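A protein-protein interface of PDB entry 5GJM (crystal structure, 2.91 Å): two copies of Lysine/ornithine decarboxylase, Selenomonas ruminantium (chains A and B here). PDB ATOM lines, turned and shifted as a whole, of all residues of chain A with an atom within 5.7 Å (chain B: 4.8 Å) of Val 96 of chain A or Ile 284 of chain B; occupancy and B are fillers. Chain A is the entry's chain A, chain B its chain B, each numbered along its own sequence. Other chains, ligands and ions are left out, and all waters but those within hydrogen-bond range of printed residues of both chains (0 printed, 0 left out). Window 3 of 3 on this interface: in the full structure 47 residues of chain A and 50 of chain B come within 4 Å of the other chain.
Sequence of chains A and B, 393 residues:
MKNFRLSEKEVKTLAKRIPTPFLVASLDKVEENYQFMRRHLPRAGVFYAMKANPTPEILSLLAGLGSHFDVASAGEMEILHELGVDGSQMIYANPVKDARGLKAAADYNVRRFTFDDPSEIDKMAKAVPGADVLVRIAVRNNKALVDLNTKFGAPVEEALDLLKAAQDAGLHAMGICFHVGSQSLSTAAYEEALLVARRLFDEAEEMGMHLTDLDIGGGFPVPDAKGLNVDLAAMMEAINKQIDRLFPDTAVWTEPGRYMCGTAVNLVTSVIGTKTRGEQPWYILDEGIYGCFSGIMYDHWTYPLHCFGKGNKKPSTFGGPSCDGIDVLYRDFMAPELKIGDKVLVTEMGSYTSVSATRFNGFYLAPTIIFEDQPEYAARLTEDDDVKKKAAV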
ATOM      1  N   TYR A  92     -16.658 -17.011  21.465  1.00  0.00           N
ATOM      2  CA  TYR A  92     -16.541 -17.909  20.354  1.00  0.00           C
ATOM      3  C   TYR A  92     -17.870 -18.627  20.263  1.00  0.00           C
ATOM      4  O   TYR A  92     -18.136 -19.598  20.940  1.00  0.00           O
ATOM      5  CB  TYR A  92     -15.389 -18.857  20.649  1.00  0.00           C
ATOM      6  CG  TYR A  92     -14.996 -19.778  19.538  1.00  0.00           C
ATOM      7  CD1 TYR A  92     -15.483 -19.608  18.270  1.00  0.00           C
ATOM      8  CD2 TYR A  92     -14.134 -20.812  19.765  1.00  0.00           C
ATOM      9  CE1 TYR A  92     -15.134 -20.457  17.261  1.00  0.00           C
ATOM     10  CE2 TYR A  92     -13.781 -21.662  18.759  1.00  0.00           C
ATOM     11  CZ  TYR A  92     -14.278 -21.472  17.510  1.00  0.00           C
ATOM     12  OH  TYR A  92     -13.944 -22.310  16.498  1.00  0.00           O
ATOM     13  N   ASN A  94     -19.599 -20.028  17.782  1.00  0.00           N
ATOM     14  CA  ASN A  94     -19.924 -21.048  16.834  1.00  0.00           C
ATOM     15  C   ASN A  94     -20.211 -22.264  17.675  1.00  0.00           C
ATOM     16  O   ASN A  94     -19.373 -22.659  18.459  1.00  0.00           O
ATOM     17  CB  ASN A  94     -18.717 -21.302  15.945  1.00  0.00           C
ATOM     18  CG  ASN A  94     -19.059 -22.102  14.727  1.00  0.00           C
ATOM     19  OD1 ASN A  94     -20.127 -22.638  14.627  1.00  0.00           O
ATOM     20  ND2 ASN A  94     -18.158 -22.179  13.805  1.00  0.00           N
ATOM     21  N   PRO A  95     -21.387 -22.864  17.532  1.00  0.00           N
ATOM     22  CA  PRO A  95     -21.689 -24.037  18.363  1.00  0.00           C
ATOM     23  C   PRO A  95     -20.887 -25.282  18.025  1.00  0.00           C
ATOM     24  O   PRO A  95     -20.751 -26.141  18.882  1.00  0.00           O
ATOM     25  CB  PRO A  95     -23.173 -24.296  18.088  1.00  0.00           C
ATOM     26  CG  PRO A  95     -23.690 -23.006  17.632  1.00  0.00           C
ATOM     27  CD  PRO A  95     -22.579 -22.448  16.785  1.00  0.00           C
ATOM     28  N   VAL A  96     -20.407 -25.400  16.784  1.00  0.00           N
ATOM     29  CA  VAL A  96     -19.517 -26.497  16.411  1.00  0.00           C
ATOM     30  C   VAL A  96     -18.180 -25.958  15.951  1.00  0.00           C
ATOM     31  O   VAL A  96     -18.050 -25.433  14.825  1.00  0.00           O
ATOM     32  CB  VAL A  96     -20.114 -27.427  15.333  1.00  0.00           C
ATOM     33  CG1 VAL A  96     -19.131 -28.548  14.982  1.00  0.00           C
ATOM     34  CG2 VAL A  96     -21.421 -28.010  15.851  1.00  0.00           C
ATOM     35  N   LYS A  97     -17.220 -26.089  16.851  1.00  0.00           N
ATOM     36  CA  LYS A  97     -15.895 -25.551  16.727  1.00  0.00           C
ATOM     37  C   LYS A  97     -14.878 -26.514  16.172  1.00  0.00           C
ATOM     38  O   LYS A  97     -15.002 -27.709  16.285  1.00  0.00           O
ATOM     39  CB  LYS A  97     -15.432 -25.069  18.077  1.00  0.00           C
ATOM     40  CG  LYS A  97     -16.398 -24.105  18.703  1.00  0.00           C
ATOM     41  CD  LYS A  97     -16.311 -24.149  20.198  1.00  0.00           C
ATOM     42  CE  LYS A  97     -17.207 -23.106  20.768  1.00  0.00           C
ATOM     43  NZ  LYS A  97     -18.585 -23.560  20.554  1.00  0.00           N
ATOM     44  N   ASP A  98     -13.841 -25.938  15.599  1.00  0.00           N
ATOM     45  CA  ASP A  98     -12.833 -26.669  14.881  1.00  0.00           C
ATOM     46  C   ASP A  98     -11.514 -26.530  15.610  1.00  0.00           C
ATOM     47  O   ASP A  98     -11.343 -25.638  16.409  1.00  0.00           O
ATOM     48  CB  ASP A  98     -12.838 -26.243  13.397  1.00  0.00           C
ATOM     49  CG  ASP A  98     -11.603 -25.504  12.958  1.00  0.00           C
ATOM     50  OD1 ASP A  98     -10.600 -26.159  12.650  1.00  0.00           O
ATOM     51  OD2 ASP A  98     -11.648 -24.270  12.885  1.00  0.00           O
ATOM     52  N   ASP A 116     -24.388 -26.370  21.767  1.00  0.00           N
ATOM     53  CA  ASP A 116     -25.747 -26.889  21.822  1.00  0.00           C
ATOM     54  C   ASP A 116     -25.851 -28.407  21.799  1.00  0.00           C
ATOM     55  O   ASP A 116     -26.938 -28.933  21.508  1.00  0.00           O
ATOM     56  CB  ASP A 116     -26.587 -26.264  20.704  1.00  0.00           C
ATOM     57  CG  ASP A 116     -26.065 -26.566  19.285  1.00  0.00           C
ATOM     58  OD1 ASP A 116     -25.475 -27.640  19.008  1.00  0.00           O
ATOM     59  OD2 ASP A 116     -26.311 -25.700  18.413  1.00  0.00           O
ATOM     60  N   GLU A 120     -19.694 -31.545  21.756  1.00  0.00           N
ATOM     61  CA  GLU A 120     -18.882 -30.335  21.908  1.00  0.00           C
ATOM     62  C   GLU A 120     -18.122 -30.195  23.246  1.00  0.00           C
ATOM     63  O   GLU A 120     -17.023 -29.644  23.262  1.00  0.00           O
ATOM     64  CB  GLU A 120     -19.766 -29.097  21.705  1.00  0.00           C
ATOM     65  CG  GLU A 120     -19.000 -27.827  21.374  1.00  0.00           C
ATOM     66  CD  GLU A 120     -18.263 -27.867  20.036  1.00  0.00           C
ATOM     67  OE1 GLU A 120     -18.454 -28.805  19.205  1.00  0.00           O
ATOM     68  OE2 GLU A 120     -17.482 -26.918  19.818  1.00  0.00           O
ATOM     69  N   LYS A 123     -14.581 -31.609  23.761  1.00  0.00           N
ATOM     70  CA  LYS A 123     -13.724 -30.861  22.841  1.00  0.00           C
ATOM     71  C   LYS A 123     -13.248 -29.516  23.445  1.00  0.00           C
ATOM     72  O   LYS A 123     -12.112 -29.098  23.208  1.00  0.00           O
ATOM     73  CB  LYS A 123     -14.485 -30.643  21.539  1.00  0.00           C
ATOM     74  CG  LYS A 123     -13.638 -30.320  20.326  1.00  0.00           C
ATOM     75  CD  LYS A 123     -14.453 -29.568  19.271  1.00  0.00           C
ATOM     76  CE  LYS A 123     -15.679 -30.345  18.792  1.00  0.00           C
ATOM     77  NZ  LYS A 123     -16.509 -29.540  17.851  1.00  0.00           N
ATOM     78  N   LYS A 151     -29.918 -26.707  12.284  1.00  0.00           N
ATOM     79  CA  LYS A 151     -28.493 -26.752  12.524  1.00  0.00           C
ATOM     80  C   LYS A 151     -28.055 -26.399  13.936  1.00  0.00           C
ATOM     81  O   LYS A 151     -27.066 -26.915  14.413  1.00  0.00           O
ATOM     82  CB  LYS A 151     -27.769 -25.892  11.516  1.00  0.00           C
ATOM     83  CG  LYS A 151     -26.503 -26.513  11.002  1.00  0.00           C
ATOM     84  CD  LYS A 151     -25.759 -25.572  10.094  1.00  0.00           C
ATOM     85  CE  LYS A 151     -24.393 -26.126   9.786  1.00  0.00           C
ATOM     86  NZ  LYS A 151     -23.364 -25.581  10.687  1.00  0.00           N
ATOM     87  N   SER B 270     -12.929 -33.620   7.596  1.00  0.00           N
ATOM     88  CA  SER B 270     -13.263 -34.418   8.784  1.00  0.00           C
ATOM     89  C   SER B 270     -14.553 -33.991   9.481  1.00  0.00           C
ATOM     90  O   SER B 270     -14.951 -32.804   9.455  1.00  0.00           O
ATOM     91  CB  SER B 270     -12.114 -34.421   9.795  1.00  0.00           C
ATOM     92  OG  SER B 270     -11.223 -33.387   9.495  1.00  0.00           O
ATOM     93  N   VAL B 271     -15.182 -34.966  10.126  1.00  0.00           N
ATOM     94  CA  VAL B 271     -16.286 -34.672  11.009  1.00  0.00           C
ATOM     95  C   VAL B 271     -15.731 -33.916  12.239  1.00  0.00           C
ATOM     96  O   VAL B 271     -14.887 -34.445  12.977  1.00  0.00           O
ATOM     97  CB  VAL B 271     -16.986 -35.960  11.454  1.00  0.00           C
ATOM     98  CG1 VAL B 271     -18.101 -35.653  12.451  1.00  0.00           C
ATOM     99  CG2 VAL B 271     -17.521 -36.696  10.241  1.00  0.00           C
ATOM    100  N   ILE B 272     -16.195 -32.679  12.431  1.00  0.00           N
ATOM    101  CA  ILE B 272     -15.804 -31.865  13.593  1.00  0.00           C
ATOM    102  C   ILE B 272     -16.844 -31.829  14.716  1.00  0.00           C
ATOM    103  O   ILE B 272     -16.490 -31.532  15.834  1.00  0.00           O
ATOM    104  CB  ILE B 272     -15.378 -30.438  13.189  1.00  0.00           C
ATOM    105  CG1 ILE B 272     -16.506 -29.672  12.483  1.00  0.00           C
ATOM    106  CG2 ILE B 272     -14.129 -30.486  12.328  1.00  0.00           C
ATOM    107  CD1 ILE B 272     -16.199 -28.205  12.323  1.00  0.00           C
ATOM    108  N   GLY B 273     -18.111 -32.119  14.412  1.00  0.00           N
ATOM    109  CA  GLY B 273     -19.165 -32.353  15.425  1.00  0.00           C
ATOM    110  C   GLY B 273     -20.201 -33.398  14.993  1.00  0.00           C
ATOM    111  O   GLY B 273     -20.307 -33.707  13.818  1.00  0.00           O
ATOM    112  N   TRP B 282     -26.704 -36.105  12.501  1.00  0.00           N
ATOM    113  CA  TRP B 282     -26.123 -34.995  11.765  1.00  0.00           C
ATOM    114  C   TRP B 282     -24.641 -34.992  11.995  1.00  0.00           C
ATOM    115  O   TRP B 282     -24.184 -35.283  13.063  1.00  0.00           O
ATOM    116  CB  TRP B 282     -26.657 -33.662  12.252  1.00  0.00           C
ATOM    117  CG  TRP B 282     -27.902 -33.177  11.643  1.00  0.00           C
ATOM    118  CD1 TRP B 282     -29.067 -33.840  11.540  1.00  0.00           C
ATOM    119  CD2 TRP B 282     -28.126 -31.885  11.099  1.00  0.00           C
ATOM    120  NE1 TRP B 282     -30.006 -33.061  10.949  1.00  0.00           N
ATOM    121  CE2 TRP B 282     -29.450 -31.844  10.671  1.00  0.00           C
ATOM    122  CE3 TRP B 282     -27.335 -30.757  10.935  1.00  0.00           C
ATOM    123  CZ2 TRP B 282     -29.993 -30.732  10.083  1.00  0.00           C
ATOM    124  CZ3 TRP B 282     -27.876 -29.671  10.353  1.00  0.00           C
ATOM    125  CH2 TRP B 282     -29.186 -29.660   9.929  1.00  0.00           C
ATOM    126  N   TYR B 283     -23.897 -34.657  10.963  1.00  0.00           N
ATOM    127  CA  TYR B 283     -22.446 -34.652  10.985  1.00  0.00           C
ATOM    128  C   TYR B 283     -21.966 -33.298  10.452  1.00  0.00           C
ATOM    129  O   TYR B 283     -22.317 -32.863   9.342  1.00  0.00           O
ATOM    130  CB  TYR B 283     -21.916 -35.822  10.146  1.00  0.00           C
ATOM    131  CG  TYR B 283     -22.298 -37.212  10.700  1.00  0.00           C
ATOM    132  CD1 TYR B 283     -21.976 -37.585  12.016  1.00  0.00           C
ATOM    133  CD2 TYR B 283     -22.975 -38.133   9.914  1.00  0.00           C
ATOM    134  CE1 TYR B 283     -22.327 -38.818  12.519  1.00  0.00           C
ATOM    135  CE2 TYR B 283     -23.316 -39.376  10.403  1.00  0.00           C
ATOM    136  CZ  TYR B 283     -22.998 -39.729  11.709  1.00  0.00           C
ATOM    137  OH  TYR B 283     -23.352 -40.999  12.187  1.00  0.00           O
ATOM    138  N   ILE B 284     -21.176 -32.609  11.255  1.00  0.00           N
ATOM    139  CA  ILE B 284     -20.602 -31.356  10.820  1.00  0.00           C
ATOM    140  C   ILE B 284     -19.208 -31.593  10.288  1.00  0.00           C
ATOM    141  O   ILE B 284     -18.336 -32.096  11.013  1.00  0.00           O
ATOM    142  CB  ILE B 284     -20.560 -30.313  11.949  1.00  0.00           C
ATOM    143  CG1 ILE B 284     -21.976 -30.109  12.540  1.00  0.00           C
ATOM    144  CG2 ILE B 284     -19.953 -29.010  11.430  1.00  0.00           C
ATOM    145  CD1 ILE B 284     -23.083 -29.833  11.529  1.00  0.00           C
ATOM    146  N   LEU B 285     -19.012 -31.215   9.023  1.00  0.00           N
ATOM    147  CA  LEU B 285     -17.701 -31.217   8.387  1.00  0.00           C
ATOM    148  C   LEU B 285     -17.055 -29.832   8.437  1.00  0.00           C
ATOM    149  O   LEU B 285     -17.731 -28.808   8.585  1.00  0.00           O
ATOM    150  CB  LEU B 285     -17.825 -31.693   6.952  1.00  0.00           C
ATOM    151  CG  LEU B 285     -18.711 -32.929   6.728  1.00  0.00           C
ATOM    152  CD1 LEU B 285     -18.756 -33.235   5.236  1.00  0.00           C
ATOM    153  CD2 LEU B 285     -18.227 -34.143   7.505  1.00  0.00           C
ATOM    154  N   ASP B 286     -15.729 -29.811   8.305  1.00  0.00           N
ATOM    155  CA  ASP B 286     -14.955 -28.551   8.349  1.00  0.00           C
ATOM    156  C   ASP B 286     -14.785 -27.889   6.983  1.00  0.00           C
ATOM    157  O   ASP B 286     -13.990 -26.974   6.856  1.00  0.00           O
ATOM    158  CB  ASP B 286     -13.599 -28.704   9.092  1.00  0.00           C
ATOM    159  CG  ASP B 286     -12.708 -29.862   8.542  1.00  0.00           C
ATOM    160  OD1 ASP B 286     -12.915 -30.317   7.389  1.00  0.00           O
ATOM    161  OD2 ASP B 286     -11.787 -30.291   9.282  1.00  0.00           O
ATOM    162  N   GLY B 319     -23.560 -31.269   7.455  1.00  0.00           N
ATOM    163  CA  GLY B 319     -23.542 -29.812   7.481  1.00  0.00           C
ATOM    164  C   GLY B 319     -22.142 -29.257   7.382  1.00  0.00           C
ATOM    165  O   GLY B 319     -21.176 -29.964   7.658  1.00  0.00           O
ATOM    166  N   GLY B 320     -22.034 -27.991   6.993  1.00  0.00           N
ATOM    167  CA  GLY B 320     -20.748 -27.321   6.973  1.00  0.00           C
ATOM    168  C   GLY B 320     -20.421 -26.631   8.293  1.00  0.00           C
ATOM    169  O   GLY B 320     -21.151 -26.762   9.270  1.00  0.00           O
ATOM    170  N   PRO B 321     -19.300 -25.902   8.331  1.00  0.00           N
ATOM    171  CA  PRO B 321     -18.744 -25.424   9.585  1.00  0.00           C
ATOM    172  C   PRO B 321     -19.201 -24.068  10.076  1.00  0.00           C
ATOM    173  O   PRO B 321     -18.816 -23.690  11.182  1.00  0.00           O
ATOM    174  CB  PRO B 321     -17.256 -25.354   9.266  1.00  0.00           C
ATOM    175  CG  PRO B 321     -17.229 -24.974   7.828  1.00  0.00           C
ATOM    176  CD  PRO B 321     -18.317 -25.808   7.238  1.00  0.00           C
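Of the 12 printed residues of chain B, 6 touch a printed residue of chain A.
Hydrophobic or aromatic side chains of chain B that line the printed part of chain A: Ile 272, Trp 282 and Ile 284.
Hydrophobic or aromatic side chains of chain A within 4 Å of the printed part of chain B: Val 96.
Among the printed residues, 7 pairs touch across the chains.
Among the printed residues, merely in contact across the chains: Lys 151 of chain A with Trp 282 of chain B (3.5 Å), Val 96 of chain A with Ile 284 of chain B (3.7 Å), Val 96 of chain A with Gly 273 of chain B (3.8 Å) and Val 96 of chain A with Ile 272 of chain B (3.8 Å).
The side-chain amide nitrogen (ND2) of Asn 94 of chain A sits at hydrogen-bond distance from the backbone carbonyl oxygen (O) of Pro 321 of chain B.
The side-chain amino group (NZ) of Lys 123 of chain A sits at hydrogen-bond distance from the backbone carbonyl oxygen (O) of Ile 272 of chain B (2.8 Å).
The backbone carbonyl oxygen (O) of Gly 320 of chain B lies within hydrogen-bond range of the side-chain amino group (NZ) of Lys 151 of chain A (2.9 Å).
The side-chain amide nitrogen (ND2) of Asn 94 of chain A sits at hydrogen-bond distance from the backbone carbonyl oxygen (O) of Val 96 of chain A (3.4 Å).
The backbone carbonyl oxygen (O) of Asn 94 of chain A is in hydrogen-bond range of the side-chain amino group (NZ) of Lys 97 of chain A (2.4 Å).
The backbone carbonyl oxygen (O) of Lys 97 of chain A is in hydrogen-bond range of the side-chain amino group (NZ) of Lys 123 of chain A.
The side-chain carboxylate (OE1) of Glu 120 of chain A is in salt-bridge range of the side-chain amino group (NZ) of Lys 123 of chain A (2.5 Å).
O of Ile 284 of chain B lies within hydrogen-bond range of N of Ile 272 of chain B, at 2.6 Å.
O of Gly 273 of chain B is in hydrogen-bond range of N of Ile 284 of chain B (2.9 Å).
No position is printed for both chains.
Of chain B, only Ile 272 (3.8 Å), Gly 273 (3.8 Å) and Ile 284 (3.7 Å) come within 4 Å of Val 96 of chain A.
Ile 284 of chain B touches just one residue of chain A: Val 96.
Printed residues of chain B within 4 Å of Asn 94 of chain A: Pro 321 (3.1 Å).
Printed residues of chain A within 4 Å of Pro 321 of chain B: Asn 94.
Printed residues of chain A within 4 Å of Trp 282 of chain B: Lys 151 (3.5 Å).
Of the printed residues of chain A, Gly 320 of chain B touches Lys 151 (2.9 Å).
The nearest residue of chain B that does not touch Val 96 of chain A is Pro 321 of chain B (4.1 Å).
The nearest printed residue of chain A that does not touch Pro 321 of chain B is Val 96 of chain A (4.1 Å).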
